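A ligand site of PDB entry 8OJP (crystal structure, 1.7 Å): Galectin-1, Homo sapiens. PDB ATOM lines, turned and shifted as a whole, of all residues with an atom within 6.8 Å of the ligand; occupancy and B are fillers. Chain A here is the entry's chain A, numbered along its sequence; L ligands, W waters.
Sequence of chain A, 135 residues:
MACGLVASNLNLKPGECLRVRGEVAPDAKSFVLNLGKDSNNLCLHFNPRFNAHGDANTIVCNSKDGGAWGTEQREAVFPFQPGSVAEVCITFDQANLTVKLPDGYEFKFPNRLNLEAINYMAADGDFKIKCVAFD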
ATOM      1  N   SER A  30       8.072  -0.777   7.860  1.00  0.00           N
ATOM      2  CA  SER A  30       7.747   0.083   6.742  1.00  0.00           C
ATOM      3  C   SER A  30       8.285  -0.553   5.470  1.00  0.00           C
ATOM      4  O   SER A  30       9.087  -1.469   5.517  1.00  0.00           O
ATOM      5  CB  SER A  30       8.279   1.504   6.903  1.00  0.00           C
ATOM      6  OG  SER A  30       9.670   1.538   6.687  1.00  0.00           O
ATOM      7  N   PHE A  31       7.801  -0.096   4.327  1.00  0.00           N
ATOM      8  CA  PHE A  31       8.442  -0.441   3.063  1.00  0.00           C
ATOM      9  C   PHE A  31       8.426   0.760   2.140  1.00  0.00           C
ATOM     10  O   PHE A  31       7.748   1.754   2.379  1.00  0.00           O
ATOM     11  CB  PHE A  31       7.805  -1.702   2.463  1.00  0.00           C
ATOM     12  CG  PHE A  31       6.403  -1.534   1.913  1.00  0.00           C
ATOM     13  CD1 PHE A  31       6.210  -1.184   0.596  1.00  0.00           C
ATOM     14  CD2 PHE A  31       5.300  -1.816   2.682  1.00  0.00           C
ATOM     15  CE1 PHE A  31       4.931  -1.079   0.063  1.00  0.00           C
ATOM     16  CE2 PHE A  31       4.023  -1.702   2.152  1.00  0.00           C
ATOM     17  CZ  PHE A  31       3.842  -1.346   0.855  1.00  0.00           C
ATOM     18  N   VAL A  32       9.206   0.644   1.035  1.00  0.00           N
ATOM     19  CA  VAL A  32       9.435   1.718   0.107  1.00  0.00           C
ATOM     20  C   VAL A  32       9.335   1.255  -1.329  1.00  0.00           C
ATOM     21  O   VAL A  32       9.858   0.205  -1.706  1.00  0.00           O
ATOM     22  CB  VAL A  32      10.838   2.279   0.345  1.00  0.00           C
ATOM     23  CG1 VAL A  32      11.223   3.286  -0.748  1.00  0.00           C
ATOM     24  CG2 VAL A  32      10.965   2.869   1.731  1.00  0.00           C
ATOM     25  N   HIS A  45       8.709   8.884  -3.814  1.00  0.00           N
ATOM     26  CA  HIS A  45       9.134   7.972  -2.777  1.00  0.00           C
ATOM     27  C   HIS A  45       7.886   7.652  -1.962  1.00  0.00           C
ATOM     28  O   HIS A  45       7.237   8.564  -1.444  1.00  0.00           O
ATOM     29  CB  HIS A  45      10.199   8.622  -1.912  1.00  0.00           C
ATOM     30  CG  HIS A  45      10.458   7.953  -0.588  1.00  0.00           C
ATOM     31  ND1 HIS A  45      11.320   6.890  -0.516  1.00  0.00           N
ATOM     32  CD2 HIS A  45      10.056   8.203   0.667  1.00  0.00           C
ATOM     33  CE1 HIS A  45      11.406   6.506   0.787  1.00  0.00           C
ATOM     34  NE2 HIS A  45      10.676   7.297   1.489  1.00  0.00           N
ATOM     35  N   ASN A  47       6.160   5.486   0.891  1.00  0.00           N
ATOM     36  CA  ASN A  47       6.676   4.877   2.120  1.00  0.00           C
ATOM     37  C   ASN A  47       5.595   4.599   3.153  1.00  0.00           C
ATOM     38  O   ASN A  47       5.400   5.397   4.072  1.00  0.00           O
ATOM     39  CB  ASN A  47       7.772   5.743   2.707  1.00  0.00           C
ATOM     40  CG  ASN A  47       8.469   5.254   3.974  1.00  0.00           C
ATOM     41  OD1 ASN A  47       8.967   6.069   4.723  1.00  0.00           O
ATOM     42  ND2 ASN A  47       8.596   3.959   4.190  1.00  0.00           N
ATOM     43  N   ARG A  49       4.309   3.352   6.429  1.00  0.00           N
ATOM     44  CA  ARG A  49       4.897   3.160   7.728  1.00  0.00           C
ATOM     45  C   ARG A  49       3.880   2.514   8.637  1.00  0.00           C
ATOM     46  O   ARG A  49       2.898   3.178   9.037  1.00  0.00           O
ATOM     47  CB  ARG A  49       5.431   4.482   8.298  1.00  0.00           C
ATOM     48  CG  ARG A  49       6.426   5.181   7.398  1.00  0.00           C
ATOM     49  CD  ARG A  49       6.756   6.606   7.837  1.00  0.00           C
ATOM     50  NE  ARG A  49       7.774   7.175   6.956  1.00  0.00           N
ATOM     51  CZ  ARG A  49       8.384   8.352   7.156  1.00  0.00           C
ATOM     52  NH1 ARG A  49       8.059   9.134   8.165  1.00  0.00           N
ATOM     53  NH2 ARG A  49       9.319   8.751   6.328  1.00  0.00           N
ATOM     54  N   ALA A  52       7.336   3.291  12.077  1.00  0.00           N
ATOM     55  CA  ALA A  52       8.657   3.616  11.596  1.00  0.00           C
ATOM     56  C   ALA A  52       8.796   5.120  11.483  1.00  0.00           C
ATOM     57  O   ALA A  52       7.821   5.810  11.167  1.00  0.00           O
ATOM     58  CB  ALA A  52       8.970   2.965  10.305  1.00  0.00           C
ATOM     59  N   HIS A  53      10.033   5.569  11.744  1.00  0.00           N
ATOM     60  CA  HIS A  53      10.490   6.897  11.364  1.00  0.00           C
ATOM     61  C   HIS A  53       9.603   7.942  12.029  1.00  0.00           C
ATOM     62  O   HIS A  53       9.454   9.029  11.485  1.00  0.00           O
ATOM     63  CB  HIS A  53      10.386   7.132   9.863  1.00  0.00           C
ATOM     64  CG  HIS A  53      11.081   6.135   9.015  1.00  0.00           C
ATOM     65  ND1 HIS A  53      12.421   5.841   9.211  1.00  0.00           N
ATOM     66  CD2 HIS A  53      10.675   5.397   8.024  1.00  0.00           C
ATOM     67  CE1 HIS A  53      12.774   4.931   8.332  1.00  0.00           C
ATOM     68  NE2 HIS A  53      11.716   4.661   7.581  1.00  0.00           N
ATOM     69  N   VAL A  60       3.712   7.908   3.972  1.00  0.00           N
ATOM     70  CA  VAL A  60       4.470   9.122   3.700  1.00  0.00           C
ATOM     71  C   VAL A  60       5.048   9.086   2.296  1.00  0.00           C
ATOM     72  O   VAL A  60       5.614   8.056   1.881  1.00  0.00           O
ATOM     73  CB  VAL A  60       5.588   9.319   4.712  1.00  0.00           C
ATOM     74  CG1 VAL A  60       6.410  10.564   4.383  1.00  0.00           C
ATOM     75  CG2 VAL A  60       5.003   9.377   6.119  1.00  0.00           C
ATOM     76  N   CYS A  61       4.724  10.132   1.534  1.00  0.00           N
ATOM     77  CA  CYS A  61       5.343  10.291   0.214  1.00  0.00           C
ATOM     78  C   CYS A  61       6.233  11.521   0.155  1.00  0.00           C
ATOM     79  O   CYS A  61       5.978  12.533   0.827  1.00  0.00           O
ATOM     80  CB  CYS A  61       4.285  10.395  -0.880  1.00  0.00           C
ATOM     81  SG  CYS A  61       3.293   8.874  -1.072  1.00  0.00           S
ATOM     82  N   ASN A  62       7.242  11.457  -0.732  1.00  0.00           N
ATOM     83  CA  ASN A  62       8.114  12.603  -0.946  1.00  0.00           C
ATOM     84  C   ASN A  62       8.681  12.489  -2.363  1.00  0.00           C
ATOM     85  O   ASN A  62       8.503  11.494  -3.056  1.00  0.00           O
ATOM     86  CB  ASN A  62       9.189  12.693   0.139  1.00  0.00           C
ATOM     87  CG  ASN A  62       9.655  14.115   0.413  1.00  0.00           C
ATOM     88  OD1 ASN A  62       9.479  15.015  -0.406  1.00  0.00           O
ATOM     89  ND2 ASN A  62      10.315  14.331   1.536  1.00  0.00           N
ATOM     90  N   SER A  63       9.411  13.524  -2.706  1.00  0.00           N
ATOM     91  CA  SER A  63      10.283  13.569  -3.877  1.00  0.00           C
ATOM     92  C   SER A  63      11.732  13.687  -3.421  1.00  0.00           C
ATOM     93  O   SER A  63      12.040  13.982  -2.270  1.00  0.00           O
ATOM     94  CB  SER A  63       9.887  14.718  -4.762  1.00  0.00           C
ATOM     95  OG  SER A  63       9.991  15.973  -4.085  1.00  0.00           O
ATOM     96  N   LYS A  64      12.640  13.508  -4.387  1.00  0.00           N
ATOM     97  CA  LYS A  64      14.038  13.738  -4.124  1.00  0.00           C
ATOM     98  C   LYS A  64      14.634  14.361  -5.376  1.00  0.00           C
ATOM     99  O   LYS A  64      14.382  13.872  -6.459  1.00  0.00           O
ATOM    100  CB  LYS A  64      14.721  12.408  -3.760  1.00  0.00           C
ATOM    101  CG  LYS A  64      16.077  12.526  -3.100  1.00  0.00           C
ATOM    102  CD  LYS A  64      16.591  11.137  -2.723  1.00  0.00           C
ATOM    103  CE  LYS A  64      17.115  11.031  -1.328  1.00  0.00           C
ATOM    104  NZ  LYS A  64      17.657   9.676  -1.119  1.00  0.00           N
ATOM    105  N   TRP A  69      15.720  15.556  -0.179  1.00  0.00           N
ATOM    106  CA  TRP A  69      14.306  15.290   0.029  1.00  0.00           C
ATOM    107  C   TRP A  69      13.492  16.575  -0.128  1.00  0.00           C
ATOM    108  O   TRP A  69      13.945  17.657   0.292  1.00  0.00           O
ATOM    109  CB  TRP A  69      14.093  14.700   1.424  1.00  0.00           C
ATOM    110  CG  TRP A  69      14.557  13.299   1.606  1.00  0.00           C
ATOM    111  CD1 TRP A  69      15.520  12.868   2.473  1.00  0.00           C
ATOM    112  CD2 TRP A  69      14.043  12.129   0.970  1.00  0.00           C
ATOM    113  NE1 TRP A  69      15.648  11.516   2.416  1.00  0.00           N
ATOM    114  CE2 TRP A  69      14.735  11.022   1.523  1.00  0.00           C
ATOM    115  CE3 TRP A  69      13.073  11.894  -0.010  1.00  0.00           C
ATOM    116  CZ2 TRP A  69      14.494   9.722   1.114  1.00  0.00           C
ATOM    117  CZ3 TRP A  69      12.845  10.607  -0.386  1.00  0.00           C
ATOM    118  CH2 TRP A  69      13.543   9.544   0.144  1.00  0.00           C
ATOM    119  N   GLY A  70      12.311  16.460  -0.719  1.00  0.00           N
ATOM    120  CA  GLY A  70      11.330  17.539  -0.786  1.00  0.00           C
ATOM    121  C   GLY A  70      10.444  17.586   0.461  1.00  0.00           C
ATOM    122  O   GLY A  70      10.831  17.172   1.552  1.00  0.00           O
ATOM    123  N   THR A  71       9.283  18.208   0.289  1.00  0.00           N
ATOM    124  CA  THR A  71       8.299  18.331   1.348  1.00  0.00           C
ATOM    125  C   THR A  71       7.464  17.056   1.438  1.00  0.00           C
ATOM    126  O   THR A  71       6.895  16.588   0.454  1.00  0.00           O
ATOM    127  CB  THR A  71       7.403  19.547   1.120  1.00  0.00           C
ATOM    128  OG1 THR A  71       8.227  20.670   0.780  1.00  0.00           O
ATOM    129  CG2 THR A  71       6.559  19.829   2.335  1.00  0.00           C
ATOM    130  N   GLU A  72       7.322  16.519   2.638  1.00  0.00           N
ATOM    131  CA  GLU A  72       6.558  15.289   2.826  1.00  0.00           C
ATOM    132  C   GLU A  72       5.062  15.557   2.618  1.00  0.00           C
ATOM    133  O   GLU A  72       4.554  16.672   2.895  1.00  0.00           O
ATOM    134  CB  GLU A  72       6.787  14.744   4.232  1.00  0.00           C
ATOM    135  CG  GLU A  72       8.206  14.293   4.440  1.00  0.00           C
ATOM    136  CD  GLU A  72       8.532  13.726   5.830  1.00  0.00           C
ATOM    137  OE1 GLU A  72       7.960  14.199   6.821  1.00  0.00           O
ATOM    138  OE2 GLU A  72       9.379  12.840   5.902  1.00  0.00           O
ATOM    139  N   GLN A  73       4.361  14.495   2.236  1.00  0.00           N
ATOM    140  CA  GLN A  73       2.926  14.469   2.079  1.00  0.00           C
ATOM    141  C   GLN A  73       2.426  13.191   2.753  1.00  0.00           C
ATOM    142  O   GLN A  73       2.960  12.106   2.511  1.00  0.00           O
ATOM    143  CB  GLN A  73       2.492  14.512   0.612  1.00  0.00           C
ATOM    144  CG  GLN A  73       0.972  14.605   0.426  1.00  0.00           C
ATOM    145  CD  GLN A  73       0.565  14.621  -1.026  1.00  0.00           C
ATOM    146  OE1 GLN A  73       1.008  15.450  -1.785  1.00  0.00           O
ATOM    147  NE2 GLN A  73      -0.246  13.651  -1.432  1.00  0.00           N
ATOM    148  N   ARG A  74       1.513  13.339   3.724  1.00  0.00           N
ATOM    149  CA  ARG A  74       0.960  12.181   4.398  1.00  0.00           C
ATOM    150  C   ARG A  74      -0.469  11.911   3.977  1.00  0.00           C
ATOM    151  O   ARG A  74      -1.270  12.846   3.872  1.00  0.00           O
ATOM    152  CB  ARG A  74       1.033  12.359   5.908  1.00  0.00           C
ATOM    153  CG  ARG A  74       2.438  12.208   6.481  1.00  0.00           C
ATOM    154  CD  ARG A  74       2.532  12.615   7.949  1.00  0.00           C
ATOM    155  NE  ARG A  74       3.802  12.156   8.523  1.00  0.00           N
ATOM    156  CZ  ARG A  74       5.001  12.636   8.201  1.00  0.00           C
ATOM    157  NH1 ARG A  74       5.093  13.701   7.447  1.00  0.00           N
ATOM    158  NH2 ARG A  74       6.116  12.103   8.684  1.00  0.00           N
ATOM    159  N   ASP A 124      12.439  -1.232  -1.285  1.00  0.00           N
ATOM    160  CA  ASP A 124      13.206  -1.424  -0.081  1.00  0.00           C
ATOM    161  C   ASP A 124      12.246  -1.731   1.077  1.00  0.00           C
ATOM    162  O   ASP A 124      11.028  -1.518   0.948  1.00  0.00           O
ATOM    163  CB  ASP A 124      14.115  -0.223   0.200  1.00  0.00           C
ATOM    164  CG  ASP A 124      15.353  -0.483   1.021  1.00  0.00           C
ATOM    165  OD1 ASP A 124      15.557  -1.652   1.460  1.00  0.00           O
ATOM    166  OD2 ASP A 124      16.107   0.491   1.267  1.00  0.00           O
ATOM    167  N   GLY A 125      12.834  -2.160   2.204  1.00  0.00           N
ATOM    168  CA  GLY A 125      12.103  -2.370   3.436  1.00  0.00           C
ATOM    169  C   GLY A 125      11.319  -3.681   3.398  1.00  0.00           C
ATOM    170  O   GLY A 125      11.712  -4.642   2.723  1.00  0.00           O
ATOM    171  N   ASP A 126      10.253  -3.718   4.198  1.00  0.00           N
ATOM    172  CA  ASP A 126       9.697  -4.973   4.663  1.00  0.00           C
ATOM    173  C   ASP A 126       8.587  -5.494   3.739  1.00  0.00           C
ATOM    174  O   ASP A 126       7.433  -5.690   4.158  1.00  0.00           O
ATOM    175  CB  ASP A 126       9.220  -4.804   6.098  1.00  0.00           C
ATOM    176  CG  ASP A 126      10.312  -4.346   7.053  1.00  0.00           C
ATOM    177  OD1 ASP A 126      11.410  -4.840   6.944  1.00  0.00           O
ATOM    178  OD2 ASP A 126      10.041  -3.490   7.871  1.00  0.00           O
HETATM  179  C1  LIG L   1      12.689   1.537   4.737  1.00  0.00           C
HETATM  180  C2  LIG L   1      12.765  13.158   7.612  1.00  0.00           C
HETATM  181  C3  LIG L   1      12.191  14.399   7.810  1.00  0.00           C
HETATM  182  C4  LIG L   1      11.888  15.258   6.742  1.00  0.00           C
HETATM  183  C5  LIG L   1      12.430  14.850   5.509  1.00  0.00           C
HETATM  184  C6  LIG L   1      13.019  13.656   5.259  1.00  0.00           C
HETATM  185  C7  LIG L   1      13.625   3.541   4.302  1.00  0.00           C
HETATM  186  C8  LIG L   1      13.267  12.831   6.363  1.00  0.00           C
HETATM  187  C9  LIG L   1      13.013   5.930   4.775  1.00  0.00           C
HETATM  188  C10 LIG L   1      13.387   8.505   4.728  1.00  0.00           C
HETATM  189  N1  LIG L   1      14.933   5.456   3.633  1.00  0.00           N
HETATM  190  C11 LIG L   1      11.772  10.308   4.143  1.00  0.00           C
HETATM  191  C12 LIG L   1      10.692  10.914   3.256  1.00  0.00           C
HETATM  192  O1  LIG L   1      10.376  12.310   3.527  1.00  0.00           O
HETATM  193  C13 LIG L   1      12.979   8.743   6.123  1.00  0.00           C
HETATM  194  F1  LIG L   1      11.288  16.467   6.904  1.00  0.00           F
HETATM  195 CL1  LIG L   1      12.045  15.911   4.162  1.00  0.00          CL
HETATM  196 CL2  LIG L   1      11.520  14.874   9.370  1.00  0.00          CL
HETATM  197  S1  LIG L   1      14.024  11.318   6.158  1.00  0.00           S
HETATM  198  C14 LIG L   1      12.637  10.179   6.360  1.00  0.00           C
HETATM  199  O2  LIG L   1      14.055   8.395   7.002  1.00  0.00           O
HETATM  200  C15 LIG L   1      12.228   8.913   3.809  1.00  0.00           C
HETATM  201  O3  LIG L   1      11.094   8.058   4.046  1.00  0.00           O
HETATM  202  O4  LIG L   1      11.583  10.528   5.511  1.00  0.00           O
HETATM  203  N2  LIG L   1      13.669   7.065   4.511  1.00  0.00           N
HETATM  204  N3  LIG L   1      14.831   6.827   3.795  1.00  0.00           N
HETATM  205  C16 LIG L   1      13.870   4.984   4.278  1.00  0.00           C
HETATM  206  S2  LIG L   1      14.645   2.489   3.430  1.00  0.00           S
HETATM  207  C17 LIG L   1      13.749   1.103   3.939  1.00  0.00           C
HETATM  208  N4  LIG L   1      12.640   2.915   4.940  1.00  0.00           N
HETATM  209  O   HOH W   1       8.105  14.571   9.499  1.00  0.00           O
HETATM  210  O   HOH W   2       9.637  11.498   8.126  1.00  0.00           O
HETATM  211  O   HOH W   3       7.929  16.846   7.259  1.00  0.00           O
HETATM  212  O   HOH W   4       9.582  12.425  10.911  1.00  0.00           O
HETATM  213  O   HOH W   5      13.799   8.683   9.560  1.00  0.00           O
HETATM  214  O   HOH W   6      16.749   8.980   6.810  1.00  0.00           O
HETATM  215  O   HOH W   7      10.919  19.197   4.510  1.00  0.00           O
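The side-chain amide nitrogen of Asn 62 lies within hydrogen-bond range of an oxygen (O1) of the ligand, 2.8 Å away. A ring nitrogen (NE2) of His 45 sits at hydrogen-bond distance from an oxygen (O3) of the ligand (2.7 Å). The side-chain amide oxygen (OD1) of Asn 47 sits at hydrogen-bond distance from an oxygen (O3) of the ligand (3.0 Å). A ring nitrogen (NE2) of His 53 is in hydrogen-bond range of a nitrogen (N4) of the ligand. The side-chain carboxylate (OE2) of Glu 72 lies within hydrogen-bond range of an oxygen (O1) of the ligand. The guanidinium group (NH2) of Arg 49 is in hydrogen-bond range of an oxygen (O3) of the ligand (3.0 Å).
The guanidinium group (NE) of Arg 49 sits at hydrogen-bond distance from the side-chain amide oxygen (OD1) of Asn 47, at 2.8 Å. The backbone carbonyl oxygen (O) of Ser 30 sits at hydrogen-bond distance from the backbone NH (N) of Asp 126. N of Gly 70 sits at hydrogen-bond distance from O of Ser 63 (2.9 Å). The guanidinium group (NH1) of Arg 74 lies within salt-bridge range of the side-chain carboxylate (OE1) of Glu 72 (3.0 Å). N of His 45 is in hydrogen-bond range of O of Asn 62 (2.7 Å). O of Gly 70 lies within hydrogen-bond range of ND2 of Asn 62, at 2.9 Å. The side-chain amide oxygen of Asn 62 sits close to the backbone carbonyl oxygen of Thr 71, at 3.1 Å. The backbone NH of Asn 47 lies within hydrogen-bond range of the backbone carbonyl oxygen of Val 60, 2.8 Å away.
OD2 of Asp 124 sits close to S2 of the ligand (3.3 Å). Residues that only touch the ligand: Gly 70 (3.1 Å), Ser 30 (3.6 Å), Trp 69 (3.6 Å), Val 32 (3.6 Å) and Gly 125 (3.8 Å). Within 4 Å of the ligand: Ser 30, Val 32, His 45, Asn 47, Arg 49, His 53, Asn 62, Trp 69, Gly 70, Glu 72, Asp 124 and Gly 125.
Water W5 bridges an oxygen (O2) of the ligand and a ring nitrogen (ND1) of His 53. Water W2 lies within hydrogen-bond range of the side-chain carboxylate of Glu 72 (2.6 Å), the guanidinium group of Arg 49 (2.8 Å) and an oxygen (O4) of the ligand (3.4 Å). Water W1 bridges the side-chain carboxylate (OE1) of Glu 72 (2.7 Å) and the guanidinium group (NH2) of Arg 74 (3.3 Å).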
